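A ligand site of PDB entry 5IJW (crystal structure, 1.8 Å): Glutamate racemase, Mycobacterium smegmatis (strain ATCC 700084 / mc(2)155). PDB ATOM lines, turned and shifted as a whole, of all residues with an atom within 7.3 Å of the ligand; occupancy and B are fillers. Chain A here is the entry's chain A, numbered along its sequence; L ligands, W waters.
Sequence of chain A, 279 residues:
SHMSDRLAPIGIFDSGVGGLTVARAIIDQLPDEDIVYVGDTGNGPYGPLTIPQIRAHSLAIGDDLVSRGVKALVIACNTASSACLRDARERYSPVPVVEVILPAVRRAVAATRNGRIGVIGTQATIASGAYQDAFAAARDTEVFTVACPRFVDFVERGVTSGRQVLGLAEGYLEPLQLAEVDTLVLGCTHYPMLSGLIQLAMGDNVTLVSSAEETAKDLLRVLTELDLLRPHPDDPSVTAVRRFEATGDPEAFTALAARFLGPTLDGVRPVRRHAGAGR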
ATOM      1  N   ASP A  14      -5.570  29.226  15.764  1.00  0.00           N
ATOM      2  CA  ASP A  14      -5.918  27.829  15.539  1.00  0.00           C
ATOM      3  C   ASP A  14      -7.330  27.596  16.064  1.00  0.00           C
ATOM      4  O   ASP A  14      -7.855  28.391  16.842  1.00  0.00           O
ATOM      5  CB  ASP A  14      -4.931  26.886  16.233  1.00  0.00           C
ATOM      6  CG  ASP A  14      -5.325  25.421  16.105  1.00  0.00           C
ATOM      7  OD1 ASP A  14      -5.414  24.954  14.958  1.00  0.00           O
ATOM      8  OD2 ASP A  14      -5.553  24.768  17.141  1.00  0.00           O
ATOM      9  N   SER A  15      -7.939  26.485  15.620  1.00  0.00           N
ATOM     10  CA  SER A  15      -9.267  26.126  16.119  1.00  0.00           C
ATOM     11  C   SER A  15      -9.270  25.881  17.619  1.00  0.00           C
ATOM     12  O   SER A  15     -10.345  25.895  18.240  1.00  0.00           O
ATOM     13  CB  SER A  15      -9.772  24.866  15.407  1.00  0.00           C
ATOM     14  OG  SER A  15      -8.961  23.764  15.791  1.00  0.00           O
ATOM     15  N   GLY A  16      -8.110  25.622  18.212  1.00  0.00           N
ATOM     16  CA  GLY A  16      -8.065  25.338  19.628  1.00  0.00           C
ATOM     17  C   GLY A  16      -6.664  25.188  20.173  1.00  0.00           C
ATOM     18  O   GLY A  16      -5.856  26.117  20.087  1.00  0.00           O
ATOM     19  N   VAL A  17      -6.367  24.021  20.748  1.00  0.00           N
ATOM     20  CA  VAL A  17      -5.124  23.777  21.465  1.00  0.00           C
ATOM     21  C   VAL A  17      -4.125  23.068  20.557  1.00  0.00           C
ATOM     22  O   VAL A  17      -2.912  23.190  20.752  1.00  0.00           O
ATOM     23  CB  VAL A  17      -5.396  22.965  22.749  1.00  0.00           C
ATOM     24  CG1 VAL A  17      -4.147  22.911  23.610  1.00  0.00           C
ATOM     25  CG2 VAL A  17      -6.567  23.577  23.528  1.00  0.00           C
ATOM     26  N   GLY A  18      -4.635  22.315  19.582  1.00  0.00           N
ATOM     27  CA  GLY A  18      -3.751  21.565  18.696  1.00  0.00           C
ATOM     28  C   GLY A  18      -2.712  22.425  17.997  1.00  0.00           C
ATOM     29  O   GLY A  18      -1.602  21.959  17.735  1.00  0.00           O
ATOM     30  N   GLY A  19      -3.057  23.671  17.678  1.00  0.00           N
ATOM     31  CA  GLY A  19      -2.139  24.580  16.988  1.00  0.00           C
ATOM     32  C   GLY A  19      -0.884  24.909  17.773  1.00  0.00           C
ATOM     33  O   GLY A  19       0.041  25.515  17.207  1.00  0.00           O
ATOM     34  N   GLY A  44     -14.644  25.783  18.248  1.00  0.00           N
ATOM     35  CA  GLY A  44     -14.252  24.575  17.557  1.00  0.00           C
ATOM     36  C   GLY A  44     -14.798  23.333  18.230  1.00  0.00           C
ATOM     37  O   GLY A  44     -15.527  23.424  19.227  1.00  0.00           O
ATOM     38  N   PRO A  45     -14.437  22.162  17.717  1.00  0.00           N
ATOM     39  CA  PRO A  45     -13.487  21.987  16.613  1.00  0.00           C
ATOM     40  C   PRO A  45     -14.026  22.392  15.254  1.00  0.00           C
ATOM     41  O   PRO A  45     -15.240  22.438  15.042  1.00  0.00           O
ATOM     42  CB  PRO A  45     -13.190  20.477  16.641  1.00  0.00           C
ATOM     43  CG  PRO A  45     -14.400  19.872  17.229  1.00  0.00           C
ATOM     44  CD  PRO A  45     -14.875  20.861  18.273  1.00  0.00           C
ATOM     45  N   TYR A  46     -13.122  22.695  14.318  1.00  0.00           N
ATOM     46  CA  TYR A  46     -13.519  23.112  12.989  1.00  0.00           C
ATOM     47  C   TYR A  46     -13.750  21.951  12.035  1.00  0.00           C
ATOM     48  O   TYR A  46     -14.477  22.099  11.051  1.00  0.00           O
ATOM     49  CB  TYR A  46     -12.473  24.037  12.372  1.00  0.00           C
ATOM     50  CG  TYR A  46     -12.319  25.424  12.975  1.00  0.00           C
ATOM     51  CD1 TYR A  46     -13.248  25.953  13.877  1.00  0.00           C
ATOM     52  CD2 TYR A  46     -11.244  26.222  12.603  1.00  0.00           C
ATOM     53  CE1 TYR A  46     -13.078  27.237  14.406  1.00  0.00           C
ATOM     54  CE2 TYR A  46     -11.069  27.492  13.131  1.00  0.00           C
ATOM     55  CZ  TYR A  46     -11.983  28.006  14.023  1.00  0.00           C
ATOM     56  OH  TYR A  46     -11.777  29.283  14.516  1.00  0.00           O
ATOM     57  N   GLY A  47     -13.120  20.808  12.298  1.00  0.00           N
ATOM     58  CA  GLY A  47     -13.150  19.667  11.396  1.00  0.00           C
ATOM     59  C   GLY A  47     -14.519  19.296  10.834  1.00  0.00           C
ATOM     60  O   GLY A  47     -14.655  19.050   9.622  1.00  0.00           O
ATOM     61  N   PRO A  48     -15.545  19.223  11.677  1.00  0.00           N
ATOM     62  CA  PRO A  48     -16.879  18.797  11.199  1.00  0.00           C
ATOM     63  C   PRO A  48     -17.765  19.922  10.705  1.00  0.00           C
ATOM     64  O   PRO A  48     -18.922  19.647  10.357  1.00  0.00           O
ATOM     65  CB  PRO A  48     -17.492  18.134  12.450  1.00  0.00           C
ATOM     66  CG  PRO A  48     -16.881  18.843  13.582  1.00  0.00           C
ATOM     67  CD  PRO A  48     -15.486  19.244  13.148  1.00  0.00           C
ATOM     68  N   LEU A  49     -17.298  21.154  10.653  1.00  0.00           N
ATOM     69  CA  LEU A  49     -18.148  22.300  10.341  1.00  0.00           C
ATOM     70  C   LEU A  49     -18.206  22.572   8.830  1.00  0.00           C
ATOM     71  O   LEU A  49     -17.494  21.954   8.030  1.00  0.00           O
ATOM     72  CB  LEU A  49     -17.649  23.547  11.072  1.00  0.00           C
ATOM     73  CG  LEU A  49     -17.582  23.472  12.598  1.00  0.00           C
ATOM     74  CD1 LEU A  49     -17.130  24.821  13.159  1.00  0.00           C
ATOM     75  CD2 LEU A  49     -18.942  23.069  13.169  1.00  0.00           C
ATOM     76  N   ALA A  76      -2.353  28.539  11.868  1.00  0.00           N
ATOM     77  CA  ALA A  76      -1.791  27.259  12.282  1.00  0.00           C
ATOM     78  C   ALA A  76      -2.718  26.101  11.996  1.00  0.00           C
ATOM     79  O   ALA A  76      -2.269  24.947  11.943  1.00  0.00           O
ATOM     80  CB  ALA A  76      -1.481  27.283  13.780  1.00  0.00           C
ATOM     81  N   CYS A  77      -4.007  26.373  11.820  1.00  0.00           N
ATOM     82  CA  CYS A  77      -5.027  25.355  11.649  1.00  0.00           C
ATOM     83  C   CYS A  77      -5.141  24.946  10.182  1.00  0.00           C
ATOM     84  O   CYS A  77      -5.376  25.803   9.315  1.00  0.00           O
ATOM     85  CB  CYS A  77      -6.374  25.899  12.153  1.00  0.00           C
ATOM     86  SG  CYS A  77      -7.765  24.725  12.002  1.00  0.00           S
ATOM     87  N   ASN A  78      -5.003  23.649   9.907  1.00  0.00           N
ATOM     88  CA  ASN A  78      -5.192  23.202   8.521  1.00  0.00           C
ATOM     89  C   ASN A  78      -6.632  23.362   8.071  1.00  0.00           C
ATOM     90  O   ASN A  78      -6.872  23.597   6.884  1.00  0.00           O
ATOM     91  CB  ASN A  78      -4.763  21.734   8.369  1.00  0.00           C
ATOM     92  CG  ASN A  78      -3.311  21.527   8.669  1.00  0.00           C
ATOM     93  OD1 ASN A  78      -2.903  21.524   9.827  1.00  0.00           O
ATOM     94  ND2 ASN A  78      -2.514  21.331   7.612  1.00  0.00           N
ATOM     95  N   THR A  79      -7.594  23.211   8.973  1.00  0.00           N
ATOM     96  CA  THR A  79      -8.991  23.363   8.564  1.00  0.00           C
ATOM     97  C   THR A  79      -9.305  24.834   8.273  1.00  0.00           C
ATOM     98  O   THR A  79      -9.934  25.140   7.256  1.00  0.00           O
ATOM     99  CB  THR A  79      -9.947  22.811   9.632  1.00  0.00           C
ATOM    100  OG1 THR A  79      -9.660  21.426   9.894  1.00  0.00           O
ATOM    101  CG2 THR A  79     -11.389  22.916   9.145  1.00  0.00           C
ATOM    102  N   ALA A  80      -8.861  25.741   9.136  1.00  0.00           N
ATOM    103  CA  ALA A  80      -9.065  27.163   8.858  1.00  0.00           C
ATOM    104  C   ALA A  80      -8.347  27.572   7.575  1.00  0.00           C
ATOM    105  O   ALA A  80      -8.918  28.289   6.751  1.00  0.00           O
ATOM    106  CB  ALA A  80      -8.566  28.016  10.035  1.00  0.00           C
ATOM    107  N   VAL A 100      -0.456  26.680   6.755  1.00  0.00           N
ATOM    108  CA  VAL A 100       0.075  25.333   6.958  1.00  0.00           C
ATOM    109  C   VAL A 100      -0.160  24.409   5.776  1.00  0.00           C
ATOM    110  O   VAL A 100       0.297  23.249   5.829  1.00  0.00           O
ATOM    111  CB  VAL A 100      -0.469  24.708   8.250  1.00  0.00           C
ATOM    112  CG1 VAL A 100       0.198  25.361   9.474  1.00  0.00           C
ATOM    113  CG2 VAL A 100      -1.997  24.863   8.364  1.00  0.00           C
ATOM    114  N   GLY A 121      -6.206  14.552   6.762  1.00  0.00           N
ATOM    115  CA  GLY A 121      -6.638  15.712   7.524  1.00  0.00           C
ATOM    116  C   GLY A 121      -8.082  15.560   7.948  1.00  0.00           C
ATOM    117  O   GLY A 121      -8.690  14.503   7.792  1.00  0.00           O
ATOM    118  N   THR A 122      -8.638  16.646   8.492  1.00  0.00           N
ATOM    119  CA  THR A 122     -10.031  16.628   8.937  1.00  0.00           C
ATOM    120  C   THR A 122     -10.957  16.509   7.747  1.00  0.00           C
ATOM    121  O   THR A 122     -10.569  16.750   6.602  1.00  0.00           O
ATOM    122  CB  THR A 122     -10.416  17.902   9.695  1.00  0.00           C
ATOM    123  OG1 THR A 122     -10.320  19.009   8.795  1.00  0.00           O
ATOM    124  CG2 THR A 122      -9.554  18.141  10.947  1.00  0.00           C
ATOM    125  N   GLN A 123     -12.219  16.174   8.034  1.00  0.00           N
ATOM    126  CA  GLN A 123     -13.243  16.143   6.994  1.00  0.00           C
ATOM    127  C   GLN A 123     -13.292  17.454   6.212  1.00  0.00           C
ATOM    128  O   GLN A 123     -13.234  17.457   4.981  1.00  0.00           O
ATOM    129  CB  GLN A 123     -14.594  15.865   7.642  1.00  0.00           C
ATOM    130  CG  GLN A 123     -15.764  15.981   6.697  1.00  0.00           C
ATOM    131  CD  GLN A 123     -17.026  15.583   7.390  1.00  0.00           C
ATOM    132  OE1 GLN A 123     -17.343  14.404   7.471  1.00  0.00           O
ATOM    133  NE2 GLN A 123     -17.716  16.558   7.974  1.00  0.00           N
ATOM    134  N   THR A 125     -11.099  19.860   5.917  1.00  0.00           N
ATOM    135  CA  THR A 125      -9.880  20.104   5.158  1.00  0.00           C
ATOM    136  C   THR A 125      -9.878  19.315   3.860  1.00  0.00           C
ATOM    137  O   THR A 125      -9.571  19.857   2.785  1.00  0.00           O
ATOM    138  CB  THR A 125      -8.668  19.744   6.021  1.00  0.00           C
ATOM    139  OG1 THR A 125      -8.550  20.685   7.084  1.00  0.00           O
ATOM    140  CG2 THR A 125      -7.386  19.773   5.178  1.00  0.00           C
ATOM    141  N   PRO A 149     -11.197  11.505  10.714  1.00  0.00           N
ATOM    142  CA  PRO A 149     -11.858  12.362  11.724  1.00  0.00           C
ATOM    143  C   PRO A 149     -11.568  11.998  13.162  1.00  0.00           C
ATOM    144  O   PRO A 149     -11.416  12.905  13.983  1.00  0.00           O
ATOM    145  CB  PRO A 149     -13.340  12.213  11.375  1.00  0.00           C
ATOM    146  CG  PRO A 149     -13.336  11.998   9.881  1.00  0.00           C
ATOM    147  CD  PRO A 149     -12.174  10.998   9.729  1.00  0.00           C
ATOM    148  N   VAL A 152      -8.157  13.221  15.856  1.00  0.00           N
ATOM    149  CA  VAL A 152      -8.075  14.359  16.785  1.00  0.00           C
ATOM    150  C   VAL A 152      -8.416  13.903  18.204  1.00  0.00           C
ATOM    151  O   VAL A 152      -7.689  14.179  19.168  1.00  0.00           O
ATOM    152  CB  VAL A 152      -8.975  15.522  16.312  1.00  0.00           C
ATOM    153  CG1 VAL A 152      -9.203  16.552  17.418  1.00  0.00           C
ATOM    154  CG2 VAL A 152      -8.371  16.245  15.092  1.00  0.00           C
ATOM    155  N   GLU A 156      -5.947  13.911  21.519  1.00  0.00           N
ATOM    156  CA  GLU A 156      -6.239  14.703  22.710  1.00  0.00           C
ATOM    157  C   GLU A 156      -6.360  13.821  23.947  1.00  0.00           C
ATOM    158  O   GLU A 156      -6.038  14.287  25.057  1.00  0.00           O
ATOM    159  CB  GLU A 156      -7.501  15.550  22.481  1.00  0.00           C
ATOM    160  CG  GLU A 156      -7.308  16.553  21.342  1.00  0.00           C
ATOM    161  CD  GLU A 156      -8.328  17.697  21.310  1.00  0.00           C
ATOM    162  OE1 GLU A 156      -9.356  17.616  22.008  1.00  0.00           O
ATOM    163  OE2 GLU A 156      -8.074  18.680  20.575  1.00  0.00           O
ATOM    164  N   GLY A 187      -1.773  16.631   7.361  1.00  0.00           N
ATOM    165  CA  GLY A 187      -2.492  17.880   7.151  1.00  0.00           C
ATOM    166  C   GLY A 187      -3.447  18.263   8.258  1.00  0.00           C
ATOM    167  O   GLY A 187      -4.576  18.669   7.996  1.00  0.00           O
ATOM    168  N   CYS A 188      -2.979  18.191   9.506  1.00  0.00           N
ATOM    169  CA  CYS A 188      -3.798  18.536  10.664  1.00  0.00           C
ATOM    170  C   CYS A 188      -2.866  18.866  11.822  1.00  0.00           C
ATOM    171  O   CYS A 188      -1.816  18.235  11.957  1.00  0.00           O
ATOM    172  CB  CYS A 188      -4.724  17.375  11.029  1.00  0.00           C
ATOM    173  SG  CYS A 188      -5.701  17.608  12.521  1.00  0.00           S
ATOM    174  N   THR A 189      -3.260  19.832  12.655  1.00  0.00           N
ATOM    175  CA  THR A 189      -2.415  20.244  13.769  1.00  0.00           C
ATOM    176  C   THR A 189      -2.062  19.080  14.681  1.00  0.00           C
ATOM    177  O   THR A 189      -0.993  19.067  15.291  1.00  0.00           O
ATOM    178  CB  THR A 189      -3.089  21.326  14.620  1.00  0.00           C
ATOM    179  OG1 THR A 189      -4.412  20.910  14.959  1.00  0.00           O
ATOM    180  CG2 THR A 189      -3.126  22.656  13.891  1.00  0.00           C
ATOM    181  N   HIS A 190      -2.982  18.128  14.828  1.00  0.00           N
ATOM    182  CA  HIS A 190      -2.792  17.098  15.840  1.00  0.00           C
ATOM    183  C   HIS A 190      -1.909  15.966  15.367  1.00  0.00           C
ATOM    184  O   HIS A 190      -1.408  15.201  16.205  1.00  0.00           O
ATOM    185  CB  HIS A 190      -4.137  16.511  16.267  1.00  0.00           C
ATOM    186  CG  HIS A 190      -5.016  17.457  17.019  1.00  0.00           C
ATOM    187  ND1 HIS A 190      -5.328  18.721  16.559  1.00  0.00           N
ATOM    188  CD2 HIS A 190      -5.667  17.312  18.200  1.00  0.00           C
ATOM    189  CE1 HIS A 190      -6.122  19.323  17.435  1.00  0.00           C
ATOM    190  NE2 HIS A 190      -6.352  18.487  18.436  1.00  0.00           N
ATOM    191  N   TYR A 191      -1.670  15.844  14.059  1.00  0.00           N
ATOM    192  CA  TYR A 191      -1.097  14.597  13.568  1.00  0.00           C
ATOM    193  C   TYR A 191       0.395  14.401  13.834  1.00  0.00           C
ATOM    194  O   TYR A 191       0.851  13.260  13.762  1.00  0.00           O
ATOM    195  CB  TYR A 191      -1.365  14.443  12.071  1.00  0.00           C
ATOM    196  CG  TYR A 191      -2.834  14.326  11.691  1.00  0.00           C
ATOM    197  CD1 TYR A 191      -3.844  14.314  12.658  1.00  0.00           C
ATOM    198  CD2 TYR A 191      -3.199  14.219  10.359  1.00  0.00           C
ATOM    199  CE1 TYR A 191      -5.203  14.210  12.288  1.00  0.00           C
ATOM    200  CE2 TYR A 191      -4.545  14.112   9.981  1.00  0.00           C
ATOM    201  CZ  TYR A 191      -5.539  14.114  10.943  1.00  0.00           C
ATOM    202  OH  TYR A 191      -6.859  14.027  10.546  1.00  0.00           O
HETATM  203  N1  LIG L   1      -6.816  22.478  14.159  1.00  0.00           N
HETATM  204  C1  LIG L   1      -7.537  21.511  13.337  1.00  0.00           C
HETATM  205  C2  LIG L   1      -6.777  21.202  12.063  1.00  0.00           C
HETATM  206  O1  LIG L   1      -7.362  20.645  11.118  1.00  0.00           O
HETATM  207  C3  LIG L   1      -7.813  20.199  14.106  1.00  0.00           C
HETATM  208  C4  LIG L   1      -8.888  20.306  15.185  1.00  0.00           C
HETATM  209  C5  LIG L   1     -10.222  20.804  14.630  1.00  0.00           C
HETATM  210  O2  LIG L   1     -10.907  20.032  13.931  1.00  0.00           O
HETATM  211  O3  LIG L   1     -10.572  21.981  14.879  1.00  0.00           O
HETATM  212  O4  LIG L   1      -5.585  21.500  11.956  1.00  0.00           O
HETATM  213  O   HOH W   1      -6.883  22.405  17.591  1.00  0.00           O
HETATM  214  O   HOH W   2     -11.849  17.545  14.360  1.00  0.00           O
HETATM  215  O   HOH W   3      -7.073  19.138   8.863  1.00  0.00           O
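An oxygen (O3) of the ligand sits at hydrogen-bond distance from the side-chain hydroxyl (OG) of Ser 15 (2.6 Å). O3 of the ligand lies within hydrogen-bond range of N of Tyr 46, 2.7 Å away. The backbone NH (N) of Thr 79 lies within hydrogen-bond range of an oxygen (O1) of the ligand (3.4 Å). The side-chain hydroxyl (OG1) of Thr 79 sits at hydrogen-bond distance from an oxygen (O1) of the ligand, 2.7 Å away. N of Gly 47 sits at hydrogen-bond distance from O2 of the ligand, 2.9 Å away. An oxygen (O4) of the ligand lies within hydrogen-bond range of the backbone NH (N) of Thr 189 (2.9 Å). OG1 of Thr 189 sits at hydrogen-bond distance from N1 of the ligand, 3.0 Å away. N1 of the ligand lies within salt-bridge range of OD1 of Asp 14, 3.0 Å away. N of Asn 78 lies within hydrogen-bond range of O4 of the ligand (3.0 Å). The side-chain amide oxygen (OD1) of Asn 78 lies close to an oxygen (O4) of the ligand (3.4 Å). The side-chain sulfur (SG) of Cys 77 lies within hydrogen-bond range of a nitrogen (N1) of the ligand, 3.3 Å away. SG of Cys 188 sits close to O1 of the ligand, 3.7 Å away.
The side-chain sulfur of Cys 77 sits close to the backbone NH of Thr 79 (3.4 Å). OG1 of Thr 79 sits at hydrogen-bond distance from OG1 of Thr 122 (2.7 Å). The side-chain hydroxyl of Thr 79 sits close to the side-chain hydroxyl of Thr 125 (3.1 Å). The side-chain carboxylate of Asp 14 is in hydrogen-bond range of the backbone NH of Gly 16 (2.9 Å). The side-chain amide nitrogen (ND2) of Asn 78 lies close to the backbone carbonyl oxygen (O) of Gly 187, 3.4 Å away. The side-chain sulfur of Cys 77 sits at hydrogen-bond distance from the backbone NH of Ala 80 (3.2 Å). The side-chain hydroxyl (OG1) of Thr 122 sits at hydrogen-bond distance from the side-chain hydroxyl (OG1) of Thr 125. The side-chain sulfur (SG) of Cys 188 sits close to the backbone NH (N) of His 190, 3.6 Å away.
Pro 45 touches the ligand (CA to O3, 3.4 Å). Thr 122 touches the ligand (CG2 to O1, 3.3 Å). His 190 touches the ligand (CE1 to C4, 3.7 Å). Hydrophobic or aromatic side chains that line the ligand: Pro 45, Tyr 46 and His 190. Within 4 Å of the ligand: Asp 14, Ser 15, Pro 45, Tyr 46, Gly 47, Cys 77, Asn 78, Thr 79, Thr 122, Cys 188, Thr 189 and His 190.
Water W3 lies within hydrogen-bond range of the backbone carbonyl oxygen (O) of Gly 187 (2.7 Å), an oxygen (O1) of the ligand (2.7 Å), the side-chain hydroxyl (OG1) of Thr 125 (2.8 Å) and the backbone NH (N) of Thr 122 (3.0 Å). Water W1 lies within hydrogen-bond range of OD2 of Asp 14, N of Gly 18, OG of Ser 15, N1 of the ligand and N of Gly 16.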
